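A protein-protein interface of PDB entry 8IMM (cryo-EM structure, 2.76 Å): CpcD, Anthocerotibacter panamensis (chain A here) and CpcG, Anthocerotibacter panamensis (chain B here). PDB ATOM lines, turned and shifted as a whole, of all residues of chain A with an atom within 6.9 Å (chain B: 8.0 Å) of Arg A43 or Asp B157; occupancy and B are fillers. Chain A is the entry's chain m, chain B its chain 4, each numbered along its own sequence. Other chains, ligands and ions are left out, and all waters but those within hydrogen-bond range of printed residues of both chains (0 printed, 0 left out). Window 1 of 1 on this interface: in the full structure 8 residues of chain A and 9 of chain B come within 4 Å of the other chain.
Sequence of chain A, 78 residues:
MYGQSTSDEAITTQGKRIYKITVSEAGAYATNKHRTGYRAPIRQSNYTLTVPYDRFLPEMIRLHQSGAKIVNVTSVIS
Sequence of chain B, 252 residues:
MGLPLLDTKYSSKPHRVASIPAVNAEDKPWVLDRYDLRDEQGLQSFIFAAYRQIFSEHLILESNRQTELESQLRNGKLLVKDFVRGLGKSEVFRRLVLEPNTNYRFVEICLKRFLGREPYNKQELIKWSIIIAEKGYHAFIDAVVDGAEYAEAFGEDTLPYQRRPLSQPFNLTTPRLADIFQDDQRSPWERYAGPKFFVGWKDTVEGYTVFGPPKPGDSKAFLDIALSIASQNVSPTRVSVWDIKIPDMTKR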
ATOM      1  N   GLU A  25       3.760  -9.448  33.704  1.00  0.00           N
ATOM      2  CA  GLU A  25       2.596 -10.022  33.032  1.00  0.00           C
ATOM      3  C   GLU A  25       2.871 -11.427  32.514  1.00  0.00           C
ATOM      4  O   GLU A  25       2.484 -11.794  31.400  1.00  0.00           O
ATOM      5  CB  GLU A  25       2.136  -9.089  31.916  1.00  0.00           C
ATOM      6  CG  GLU A  25       3.111  -8.905  30.768  1.00  0.00           C
ATOM      7  CD  GLU A  25       2.605  -7.909  29.739  1.00  0.00           C
ATOM      8  OE1 GLU A  25       1.506  -7.353  29.943  1.00  0.00           O
ATOM      9  OE2 GLU A  25       3.303  -7.682  28.729  1.00  0.00           O
ATOM     10  N   TYR A  29      -0.979 -14.291  33.253  1.00  0.00           N
ATOM     11  CA  TYR A  29      -1.740 -13.139  32.782  1.00  0.00           C
ATOM     12  C   TYR A  29      -2.014 -13.240  31.285  1.00  0.00           C
ATOM     13  O   TYR A  29      -3.097 -12.862  30.816  1.00  0.00           O
ATOM     14  CB  TYR A  29      -0.985 -11.851  33.122  1.00  0.00           C
ATOM     15  CG  TYR A  29      -1.516 -10.591  32.469  1.00  0.00           C
ATOM     16  CD1 TYR A  29      -1.056 -10.178  31.224  1.00  0.00           C
ATOM     17  CD2 TYR A  29      -2.465  -9.806  33.109  1.00  0.00           C
ATOM     18  CE1 TYR A  29      -1.533  -9.025  30.632  1.00  0.00           C
ATOM     19  CE2 TYR A  29      -2.951  -8.652  32.522  1.00  0.00           C
ATOM     20  CZ  TYR A  29      -2.480  -8.267  31.284  1.00  0.00           C
ATOM     21  OH  TYR A  29      -2.959  -7.119  30.694  1.00  0.00           O
ATOM     22  N   TYR A  38      -8.188  -9.257  23.893  1.00  0.00           N
ATOM     23  CA  TYR A  38      -7.403  -8.035  24.032  1.00  0.00           C
ATOM     24  C   TYR A  38      -8.252  -6.847  23.596  1.00  0.00           C
ATOM     25  O   TYR A  38      -8.497  -6.655  22.400  1.00  0.00           O
ATOM     26  CB  TYR A  38      -6.118  -8.109  23.209  1.00  0.00           C
ATOM     27  CG  TYR A  38      -5.106  -9.102  23.726  1.00  0.00           C
ATOM     28  CD1 TYR A  38      -4.367  -8.831  24.868  1.00  0.00           C
ATOM     29  CD2 TYR A  38      -4.876 -10.302  23.067  1.00  0.00           C
ATOM     30  CE1 TYR A  38      -3.436  -9.728  25.346  1.00  0.00           C
ATOM     31  CE2 TYR A  38      -3.944 -11.209  23.538  1.00  0.00           C
ATOM     32  CZ  TYR A  38      -3.226 -10.916  24.679  1.00  0.00           C
ATOM     33  OH  TYR A  38      -2.297 -11.809  25.160  1.00  0.00           O
ATOM     34  N   ALA A  40      -7.214  -3.805  24.228  1.00  0.00           N
ATOM     35  CA  ALA A  40      -6.190  -2.815  23.946  1.00  0.00           C
ATOM     36  C   ALA A  40      -4.958  -3.523  23.409  1.00  0.00           C
ATOM     37  O   ALA A  40      -4.773  -4.722  23.643  1.00  0.00           O
ATOM     38  CB  ALA A  40      -5.832  -2.010  25.204  1.00  0.00           C
ATOM     39  N   PRO A  41      -4.105  -2.816  22.666  1.00  0.00           N
ATOM     40  CA  PRO A  41      -2.873  -3.440  22.173  1.00  0.00           C
ATOM     41  C   PRO A  41      -1.986  -3.913  23.316  1.00  0.00           C
ATOM     42  O   PRO A  41      -1.951  -3.318  24.396  1.00  0.00           O
ATOM     43  CB  PRO A  41      -2.201  -2.323  21.364  1.00  0.00           C
ATOM     44  CG  PRO A  41      -2.887  -1.061  21.791  1.00  0.00           C
ATOM     45  CD  PRO A  41      -4.284  -1.463  22.118  1.00  0.00           C
ATOM     46  N   ILE A  42      -1.271  -5.005  23.063  1.00  0.00           N
ATOM     47  CA  ILE A  42      -0.446  -5.656  24.074  1.00  0.00           C
ATOM     48  C   ILE A  42       0.812  -4.834  24.312  1.00  0.00           C
ATOM     49  O   ILE A  42       1.455  -4.365  23.367  1.00  0.00           O
ATOM     50  CB  ILE A  42      -0.108  -7.091  23.632  1.00  0.00           C
ATOM     51  CG1 ILE A  42      -1.387  -7.834  23.240  1.00  0.00           C
ATOM     52  CG2 ILE A  42       0.606  -7.837  24.745  1.00  0.00           C
ATOM     53  CD1 ILE A  42      -1.152  -9.121  22.481  1.00  0.00           C
ATOM     54  N   ARG A  43       1.172  -4.659  25.581  1.00  0.00           N
ATOM     55  CA  ARG A  43       2.316  -3.850  25.978  1.00  0.00           C
ATOM     56  C   ARG A  43       3.469  -4.730  26.447  1.00  0.00           C
ATOM     57  O   ARG A  43       3.412  -5.962  26.400  1.00  0.00           O
ATOM     58  CB  ARG A  43       1.930  -2.862  27.083  1.00  0.00           C
ATOM     59  CG  ARG A  43       1.583  -3.519  28.409  1.00  0.00           C
ATOM     60  CD  ARG A  43       1.216  -2.481  29.451  1.00  0.00           C
ATOM     61  NE  ARG A  43       0.006  -1.755  29.092  1.00  0.00           N
ATOM     62  CZ  ARG A  43      -0.007  -0.487  28.691  1.00  0.00           C
ATOM     63  NH1 ARG A  43       1.129   0.190  28.601  1.00  0.00           N
ATOM     64  NH2 ARG A  43      -1.151   0.104  28.379  1.00  0.00           N
ATOM     65  N   GLN A  44       4.529  -4.067  26.908  1.00  0.00           N
ATOM     66  CA  GLN A  44       5.719  -4.761  27.377  1.00  0.00           C
ATOM     67  C   GLN A  44       5.467  -5.451  28.714  1.00  0.00           C
ATOM     68  O   GLN A  44       4.491  -5.168  29.415  1.00  0.00           O
ATOM     69  CB  GLN A  44       6.890  -3.784  27.497  1.00  0.00           C
ATOM     70  CG  GLN A  44       7.259  -3.025  26.213  1.00  0.00           C
ATOM     71  CD  GLN A  44       7.589  -3.915  25.009  1.00  0.00           C
ATOM     72  OE1 GLN A  44       6.848  -4.834  24.654  1.00  0.00           O
ATOM     73  NE2 GLN A  44       8.717  -3.628  24.372  1.00  0.00           N
ATOM     74  N   SER A  45       6.373  -6.368  29.062  1.00  0.00           N
ATOM     75  CA  SER A  45       6.140  -7.271  30.185  1.00  0.00           C
ATOM     76  C   SER A  45       6.118  -6.531  31.518  1.00  0.00           C
ATOM     77  O   SER A  45       5.184  -6.695  32.313  1.00  0.00           O
ATOM     78  CB  SER A  45       7.206  -8.367  30.203  1.00  0.00           C
ATOM     79  OG  SER A  45       8.451  -7.862  30.653  1.00  0.00           O
ATOM     80  N   ASN A  46       7.134  -5.717  31.782  1.00  0.00           N
ATOM     81  CA  ASN A  46       7.344  -5.156  33.110  1.00  0.00           C
ATOM     82  C   ASN A  46       7.124  -3.650  33.103  1.00  0.00           C
ATOM     83  O   ASN A  46       7.534  -2.960  32.164  1.00  0.00           O
ATOM     84  CB  ASN A  46       8.756  -5.475  33.601  1.00  0.00           C
ATOM     85  CG  ASN A  46       8.969  -6.954  33.833  1.00  0.00           C
ATOM     86  OD1 ASN A  46       8.048  -7.756  33.687  1.00  0.00           O
ATOM     87  ND2 ASN A  46      10.192  -7.326  34.190  1.00  0.00           N
ATOM     88  N   TYR A  47       6.485  -3.144  34.157  1.00  0.00           N
ATOM     89  CA  TYR A  47       6.329  -1.709  34.329  1.00  0.00           C
ATOM     90  C   TYR A  47       6.197  -1.390  35.811  1.00  0.00           C
ATOM     91  O   TYR A  47       5.591  -2.144  36.576  1.00  0.00           O
ATOM     92  CB  TYR A  47       5.126  -1.174  33.544  1.00  0.00           C
ATOM     93  CG  TYR A  47       3.827  -1.896  33.817  1.00  0.00           C
ATOM     94  CD1 TYR A  47       3.030  -1.553  34.899  1.00  0.00           C
ATOM     95  CD2 TYR A  47       3.402  -2.924  32.993  1.00  0.00           C
ATOM     96  CE1 TYR A  47       1.846  -2.213  35.149  1.00  0.00           C
ATOM     97  CE2 TYR A  47       2.220  -3.590  33.234  1.00  0.00           C
ATOM     98  CZ  TYR A  47       1.446  -3.231  34.313  1.00  0.00           C
ATOM     99  OH  TYR A  47       0.267  -3.894  34.554  1.00  0.00           O
ATOM    100  N   VAL B  31      -9.366   6.206  19.240  1.00  0.00           N
ATOM    101  CA  VAL B  31      -9.114   5.466  20.469  1.00  0.00           C
ATOM    102  C   VAL B  31      -7.680   5.796  20.868  1.00  0.00           C
ATOM    103  O   VAL B  31      -6.727   5.128  20.468  1.00  0.00           O
ATOM    104  CB  VAL B  31      -9.344   3.969  20.280  1.00  0.00           C
ATOM    105  CG1 VAL B  31      -9.190   3.234  21.584  1.00  0.00           C
ATOM    106  CG2 VAL B  31     -10.722   3.730  19.696  1.00  0.00           C
ATOM    107  N   LEU B  32      -7.526   6.848  21.665  1.00  0.00           N
ATOM    108  CA  LEU B  32      -6.209   7.312  22.064  1.00  0.00           C
ATOM    109  C   LEU B  32      -5.721   6.516  23.266  1.00  0.00           C
ATOM    110  O   LEU B  32      -6.482   6.220  24.188  1.00  0.00           O
ATOM    111  CB  LEU B  32      -6.262   8.798  22.397  1.00  0.00           C
ATOM    112  CG  LEU B  32      -6.422   9.720  21.189  1.00  0.00           C
ATOM    113  CD1 LEU B  32      -6.836  11.072  21.647  1.00  0.00           C
ATOM    114  CD2 LEU B  32      -5.176   9.835  20.340  1.00  0.00           C
ATOM    115  N   ASP B  33      -4.435   6.175  23.259  1.00  0.00           N
ATOM    116  CA  ASP B  33      -3.907   5.199  24.199  1.00  0.00           C
ATOM    117  C   ASP B  33      -2.550   5.654  24.716  1.00  0.00           C
ATOM    118  O   ASP B  33      -2.119   6.785  24.492  1.00  0.00           O
ATOM    119  CB  ASP B  33      -3.807   3.820  23.549  1.00  0.00           C
ATOM    120  CG  ASP B  33      -5.084   3.027  23.662  1.00  0.00           C
ATOM    121  OD1 ASP B  33      -5.593   2.892  24.791  1.00  0.00           O
ATOM    122  OD2 ASP B  33      -5.583   2.539  22.626  1.00  0.00           O
ATOM    123  N   ARG B  34      -1.875   4.733  25.409  1.00  0.00           N
ATOM    124  CA  ARG B  34      -0.624   5.052  26.093  1.00  0.00           C
ATOM    125  C   ARG B  34       0.508   5.326  25.113  1.00  0.00           C
ATOM    126  O   ARG B  34       1.361   6.185  25.365  1.00  0.00           O
ATOM    127  CB  ARG B  34      -0.253   3.911  27.037  1.00  0.00           C
ATOM    128  CG  ARG B  34       0.978   4.169  27.875  1.00  0.00           C
ATOM    129  CD  ARG B  34       0.903   3.429  29.202  1.00  0.00           C
ATOM    130  NE  ARG B  34       0.260   4.210  30.260  1.00  0.00           N
ATOM    131  CZ  ARG B  34       0.698   5.379  30.724  1.00  0.00           C
ATOM    132  NH1 ARG B  34       0.032   5.999  31.685  1.00  0.00           N
ATOM    133  NH2 ARG B  34       1.816   5.917  30.257  1.00  0.00           N
ATOM    134  N   TYR B  35       0.540   4.608  23.991  1.00  0.00           N
ATOM    135  CA  TYR B  35       1.606   4.810  23.014  1.00  0.00           C
ATOM    136  C   TYR B  35       1.592   6.218  22.426  1.00  0.00           C
ATOM    137  O   TYR B  35       2.580   6.645  21.817  1.00  0.00           O
ATOM    138  CB  TYR B  35       1.512   3.748  21.919  1.00  0.00           C
ATOM    139  CG  TYR B  35       0.118   3.555  21.368  1.00  0.00           C
ATOM    140  CD1 TYR B  35      -0.451   4.481  20.513  1.00  0.00           C
ATOM    141  CD2 TYR B  35      -0.622   2.424  21.694  1.00  0.00           C
ATOM    142  CE1 TYR B  35      -1.728   4.306  20.017  1.00  0.00           C
ATOM    143  CE2 TYR B  35      -1.891   2.233  21.193  1.00  0.00           C
ATOM    144  CZ  TYR B  35      -2.443   3.178  20.356  1.00  0.00           C
ATOM    145  OH  TYR B  35      -3.711   2.994  19.856  1.00  0.00           O
ATOM    146  N   ASP B  36       0.489   6.949  22.584  1.00  0.00           N
ATOM    147  CA  ASP B  36       0.458   8.361  22.220  1.00  0.00           C
ATOM    148  C   ASP B  36       1.226   9.230  23.203  1.00  0.00           C
ATOM    149  O   ASP B  36       1.593  10.358  22.858  1.00  0.00           O
ATOM    150  CB  ASP B  36      -0.988   8.835  22.135  1.00  0.00           C
ATOM    151  CG  ASP B  36      -1.814   7.979  21.216  1.00  0.00           C
ATOM    152  OD1 ASP B  36      -1.221   7.306  20.354  1.00  0.00           O
ATOM    153  OD2 ASP B  36      -3.052   8.006  21.321  1.00  0.00           O
ATOM    154  N   LEU B  37       1.470   8.738  24.415  1.00  0.00           N
ATOM    155  CA  LEU B  37       2.075   9.561  25.452  1.00  0.00           C
ATOM    156  C   LEU B  37       3.583   9.700  25.279  1.00  0.00           C
ATOM    157  O   LEU B  37       4.194  10.571  25.908  1.00  0.00           O
ATOM    158  CB  LEU B  37       1.759   8.971  26.829  1.00  0.00           C
ATOM    159  CG  LEU B  37       0.420   9.295  27.493  1.00  0.00           C
ATOM    160  CD1 LEU B  37      -0.721   8.607  26.791  1.00  0.00           C
ATOM    161  CD2 LEU B  37       0.458   8.881  28.951  1.00  0.00           C
ATOM    162  N   ARG B  38       4.199   8.863  24.443  1.00  0.00           N
ATOM    163  CA  ARG B  38       5.657   8.826  24.386  1.00  0.00           C
ATOM    164  C   ARG B  38       6.226  10.004  23.601  1.00  0.00           C
ATOM    165  O   ARG B  38       7.257  10.571  23.980  1.00  0.00           O
ATOM    166  CB  ARG B  38       6.109   7.492  23.797  1.00  0.00           C
ATOM    167  CG  ARG B  38       5.937   6.350  24.783  1.00  0.00           C
ATOM    168  CD  ARG B  38       6.353   5.010  24.213  1.00  0.00           C
ATOM    169  NE  ARG B  38       6.373   3.980  25.249  1.00  0.00           N
ATOM    170  CZ  ARG B  38       5.290   3.357  25.706  1.00  0.00           C
ATOM    171  NH1 ARG B  38       5.401   2.433  26.650  1.00  0.00           N
ATOM    172  NH2 ARG B  38       4.095   3.661  25.219  1.00  0.00           N
ATOM    173  N   PHE B  46      -2.985  14.302  22.893  1.00  0.00           N
ATOM    174  CA  PHE B  46      -3.717  13.512  23.874  1.00  0.00           C
ATOM    175  C   PHE B  46      -4.300  14.395  24.966  1.00  0.00           C
ATOM    176  O   PHE B  46      -5.441  14.195  25.396  1.00  0.00           O
ATOM    177  CB  PHE B  46      -2.801  12.460  24.487  1.00  0.00           C
ATOM    178  CG  PHE B  46      -3.420  11.708  25.619  1.00  0.00           C
ATOM    179  CD1 PHE B  46      -3.381  12.205  26.907  1.00  0.00           C
ATOM    180  CD2 PHE B  46      -4.022  10.494  25.404  1.00  0.00           C
ATOM    181  CE1 PHE B  46      -3.952  11.517  27.944  1.00  0.00           C
ATOM    182  CE2 PHE B  46      -4.583   9.802  26.440  1.00  0.00           C
ATOM    183  CZ  PHE B  46      -4.549  10.318  27.709  1.00  0.00           C
ATOM    184  N   LEU B  78       1.391   8.380  35.890  1.00  0.00           N
ATOM    185  CA  LEU B  78      -0.051   8.537  35.973  1.00  0.00           C
ATOM    186  C   LEU B  78      -0.714   7.748  34.859  1.00  0.00           C
ATOM    187  O   LEU B  78      -0.348   7.892  33.691  1.00  0.00           O
ATOM    188  CB  LEU B  78      -0.427  10.014  35.876  1.00  0.00           C
ATOM    189  CG  LEU B  78      -1.763  10.454  36.452  1.00  0.00           C
ATOM    190  CD1 LEU B  78      -1.709  10.334  37.946  1.00  0.00           C
ATOM    191  CD2 LEU B  78      -2.012  11.886  36.067  1.00  0.00           C
ATOM    192  N   LEU B  79      -1.684   6.918  35.221  1.00  0.00           N
ATOM    193  CA  LEU B  79      -2.489   6.224  34.235  1.00  0.00           C
ATOM    194  C   LEU B  79      -3.458   7.196  33.575  1.00  0.00           C
ATOM    195  O   LEU B  79      -3.806   8.239  34.131  1.00  0.00           O
ATOM    196  CB  LEU B  79      -3.254   5.075  34.882  1.00  0.00           C
ATOM    197  CG  LEU B  79      -2.445   3.869  35.339  1.00  0.00           C
ATOM    198  CD1 LEU B  79      -3.206   3.111  36.399  1.00  0.00           C
ATOM    199  CD2 LEU B  79      -2.139   2.973  34.163  1.00  0.00           C
ATOM    200  N   VAL B  80      -3.897   6.846  32.370  1.00  0.00           N
ATOM    201  CA  VAL B  80      -4.874   7.681  31.685  1.00  0.00           C
ATOM    202  C   VAL B  80      -6.173   7.723  32.474  1.00  0.00           C
ATOM    203  O   VAL B  80      -6.849   8.758  32.533  1.00  0.00           O
ATOM    204  CB  VAL B  80      -5.089   7.176  30.252  1.00  0.00           C
ATOM    205  CG1 VAL B  80      -6.234   7.909  29.603  1.00  0.00           C
ATOM    206  CG2 VAL B  80      -3.824   7.347  29.457  1.00  0.00           C
ATOM    207  N   LYS B  81      -6.531   6.608  33.107  1.00  0.00           N
ATOM    208  CA  LYS B  81      -7.695   6.593  33.982  1.00  0.00           C
ATOM    209  C   LYS B  81      -7.532   7.578  35.124  1.00  0.00           C
ATOM    210  O   LYS B  81      -8.472   8.298  35.472  1.00  0.00           O
ATOM    211  CB  LYS B  81      -7.920   5.186  34.523  1.00  0.00           C
ATOM    212  CG  LYS B  81      -9.111   5.062  35.429  1.00  0.00           C
ATOM    213  CD  LYS B  81      -9.329   3.627  35.842  1.00  0.00           C
ATOM    214  CE  LYS B  81      -8.284   3.197  36.837  1.00  0.00           C
ATOM    215  NZ  LYS B  81      -8.559   1.837  37.357  1.00  0.00           N
ATOM    216  N   ASP B  82      -6.340   7.633  35.716  1.00  0.00           N
ATOM    217  CA  ASP B  82      -6.099   8.574  36.801  1.00  0.00           C
ATOM    218  C   ASP B  82      -6.101  10.012  36.310  1.00  0.00           C
ATOM    219  O   ASP B  82      -6.536  10.905  37.037  1.00  0.00           O
ATOM    220  CB  ASP B  82      -4.782   8.249  37.489  1.00  0.00           C
ATOM    221  CG  ASP B  82      -4.807   6.901  38.169  1.00  0.00           C
ATOM    222  OD1 ASP B  82      -5.858   6.542  38.734  1.00  0.00           O
ATOM    223  OD2 ASP B  82      -3.781   6.194  38.134  1.00  0.00           O
ATOM    224  N   TYR B 150     -16.666   1.104  32.853  1.00  0.00           N
ATOM    225  CA  TYR B 150     -15.501   1.844  32.391  1.00  0.00           C
ATOM    226  C   TYR B 150     -14.312   0.922  32.182  1.00  0.00           C
ATOM    227  O   TYR B 150     -13.576   1.061  31.202  1.00  0.00           O
ATOM    228  CB  TYR B 150     -15.156   2.953  33.382  1.00  0.00           C
ATOM    229  CG  TYR B 150     -13.984   3.810  32.970  1.00  0.00           C
ATOM    230  CD1 TYR B 150     -12.688   3.422  33.239  1.00  0.00           C
ATOM    231  CD2 TYR B 150     -14.177   5.008  32.320  1.00  0.00           C
ATOM    232  CE1 TYR B 150     -11.627   4.193  32.869  1.00  0.00           C
ATOM    233  CE2 TYR B 150     -13.117   5.785  31.949  1.00  0.00           C
ATOM    234  CZ  TYR B 150     -11.845   5.370  32.222  1.00  0.00           C
ATOM    235  OH  TYR B 150     -10.772   6.141  31.857  1.00  0.00           O
ATOM    236  N   ALA B 151     -14.095  -0.018  33.100  1.00  0.00           N
ATOM    237  CA  ALA B 151     -12.973  -0.935  32.955  1.00  0.00           C
ATOM    238  C   ALA B 151     -13.124  -1.791  31.709  1.00  0.00           C
ATOM    239  O   ALA B 151     -12.135  -2.107  31.042  1.00  0.00           O
ATOM    240  CB  ALA B 151     -12.842  -1.813  34.194  1.00  0.00           C
ATOM    241  N   PHE B 154     -13.002   0.990  28.282  1.00  0.00           N
ATOM    242  CA  PHE B 154     -11.774   1.722  28.006  1.00  0.00           C
ATOM    243  C   PHE B 154     -10.551   1.147  28.696  1.00  0.00           C
ATOM    244  O   PHE B 154      -9.527   0.952  28.046  1.00  0.00           O
ATOM    245  CB  PHE B 154     -11.946   3.190  28.399  1.00  0.00           C
ATOM    246  CG  PHE B 154     -13.212   3.802  27.883  1.00  0.00           C
ATOM    247  CD1 PHE B 154     -13.397   3.998  26.539  1.00  0.00           C
ATOM    248  CD2 PHE B 154     -14.214   4.181  28.740  1.00  0.00           C
ATOM    249  CE1 PHE B 154     -14.561   4.552  26.066  1.00  0.00           C
ATOM    250  CE2 PHE B 154     -15.367   4.735  28.266  1.00  0.00           C
ATOM    251  CZ  PHE B 154     -15.538   4.921  26.927  1.00  0.00           C
ATOM    252  N   GLY B 155     -10.624   0.854  29.982  1.00  0.00           N
ATOM    253  CA  GLY B 155      -9.471   0.346  30.687  1.00  0.00           C
ATOM    254  C   GLY B 155      -8.589   1.457  31.213  1.00  0.00           C
ATOM    255  O   GLY B 155      -8.910   2.644  31.153  1.00  0.00           O
ATOM    256  N   GLU B 156      -7.435   1.053  31.746  1.00  0.00           N
ATOM    257  CA  GLU B 156      -6.565   2.007  32.423  1.00  0.00           C
ATOM    258  C   GLU B 156      -5.742   2.839  31.452  1.00  0.00           C
ATOM    259  O   GLU B 156      -5.179   3.863  31.851  1.00  0.00           O
ATOM    260  CB  GLU B 156      -5.635   1.281  33.390  1.00  0.00           C
ATOM    261  CG  GLU B 156      -6.337   0.600  34.543  1.00  0.00           C
ATOM    262  CD  GLU B 156      -6.769  -0.811  34.218  1.00  0.00           C
ATOM    263  OE1 GLU B 156      -6.718  -1.192  33.029  1.00  0.00           O
ATOM    264  OE2 GLU B 156      -7.154  -1.543  35.153  1.00  0.00           O
ATOM    265  N   ASP B 157      -5.633   2.424  30.196  1.00  0.00           N
ATOM    266  CA  ASP B 157      -4.724   3.119  29.296  1.00  0.00           C
ATOM    267  C   ASP B 157      -5.432   3.858  28.172  1.00  0.00           C
ATOM    268  O   ASP B 157      -4.779   4.600  27.434  1.00  0.00           O
ATOM    269  CB  ASP B 157      -3.713   2.137  28.705  1.00  0.00           C
ATOM    270  CG  ASP B 157      -4.371   0.942  28.048  1.00  0.00           C
ATOM    271  OD1 ASP B 157      -5.508   0.596  28.432  1.00  0.00           O
ATOM    272  OD2 ASP B 157      -3.747   0.341  27.150  1.00  0.00           O
ATOM    273  N   THR B 158      -6.734   3.672  28.012  1.00  0.00           N
ATOM    274  CA  THR B 158      -7.460   4.335  26.943  1.00  0.00           C
ATOM    275  C   THR B 158      -8.205   5.550  27.471  1.00  0.00           C
ATOM    276  O   THR B 158      -8.693   5.565  28.602  1.00  0.00           O
ATOM    277  CB  THR B 158      -8.445   3.377  26.280  1.00  0.00           C
ATOM    278  OG1 THR B 158      -7.777   2.148  25.980  1.00  0.00           O
ATOM    279  CG2 THR B 158      -8.961   3.963  25.000  1.00  0.00           C
ATOM    280  N   LEU B 159      -8.272   6.574  26.644  1.00  0.00           N
ATOM    281  CA  LEU B 159      -9.014   7.791  26.913  1.00  0.00           C
ATOM    282  C   LEU B 159     -10.441   7.652  26.402  1.00  0.00           C
ATOM    283  O   LEU B 159     -10.650   7.236  25.262  1.00  0.00           O
ATOM    284  CB  LEU B 159      -8.334   8.982  26.256  1.00  0.00           C
ATOM    285  CG  LEU B 159      -8.844  10.396  26.477  1.00  0.00           C
ATOM    286  CD1 LEU B 159      -7.682  11.326  26.452  1.00  0.00           C
ATOM    287  CD2 LEU B 159      -9.777  10.761  25.360  1.00  0.00           C
ATOM    288  N   PRO B 160     -11.418   7.995  27.236  1.00  0.00           N
ATOM    289  CA  PRO B 160     -12.816   7.781  26.865  1.00  0.00           C
ATOM    290  C   PRO B 160     -13.185   8.476  25.569  1.00  0.00           C
ATOM    291  O   PRO B 160     -12.720   9.574  25.267  1.00  0.00           O
ATOM    292  CB  PRO B 160     -13.580   8.367  28.049  1.00  0.00           C
ATOM    293  CG  PRO B 160     -12.661   8.227  29.174  1.00  0.00           C
ATOM    294  CD  PRO B 160     -11.286   8.403  28.639  1.00  0.00           C
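NH2 of Arg A43 is in salt-bridge range of OD2 of Asp B157, 2.9 Å away.
The side-chain carboxylate of Asp B33 is in hydrogen-bond range of the side-chain hydroxyl of Tyr B35.
The backbone carbonyl oxygen of Leu B78 is in hydrogen-bond range of the guanidinium group of Arg B34.
Among the printed residues, merely in contact across the chains: Ala A40 with Asp B157 (3.7 Å), Pro A41 with Tyr B35 (3.5 Å) and Arg A43 with Arg B34 (3.3 Å).
Of the printed residues of chain B, Ala A40 touches Asp B157 (3.7 Å).
Of the printed residues of chain B, Pro A41 touches Tyr B35 (3.5 Å).
Of chain B, only Arg B34 and Asp B157 come within 4 Å of Arg A43.
Of the printed residues of chain A, Arg B34 touches Arg A43.
Printed residues of chain A within 4 Å of Tyr B35: Pro A41.
Of chain A, only Ala A40 (3.7 Å) and Arg A43 (2.9 Å) come within 4 Å of Asp B157.
Hydrophobic or aromatic side chains of chain A within 4 Å of the printed part of chain B: Ala A40 and Pro A41.
Of the 23 printed residues of chain B, 3 touch a printed residue of chain A.
Printed residues of chain B that touch a printed residue of chain A: Arg B34, Tyr B35 and Asp B157.
Hydrophobic or aromatic side chains of chain B within 4 Å of the printed part of chain A: Tyr B35.
Along chain B the printed residues that touch a printed residue of chain A span positions 34 to 157.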
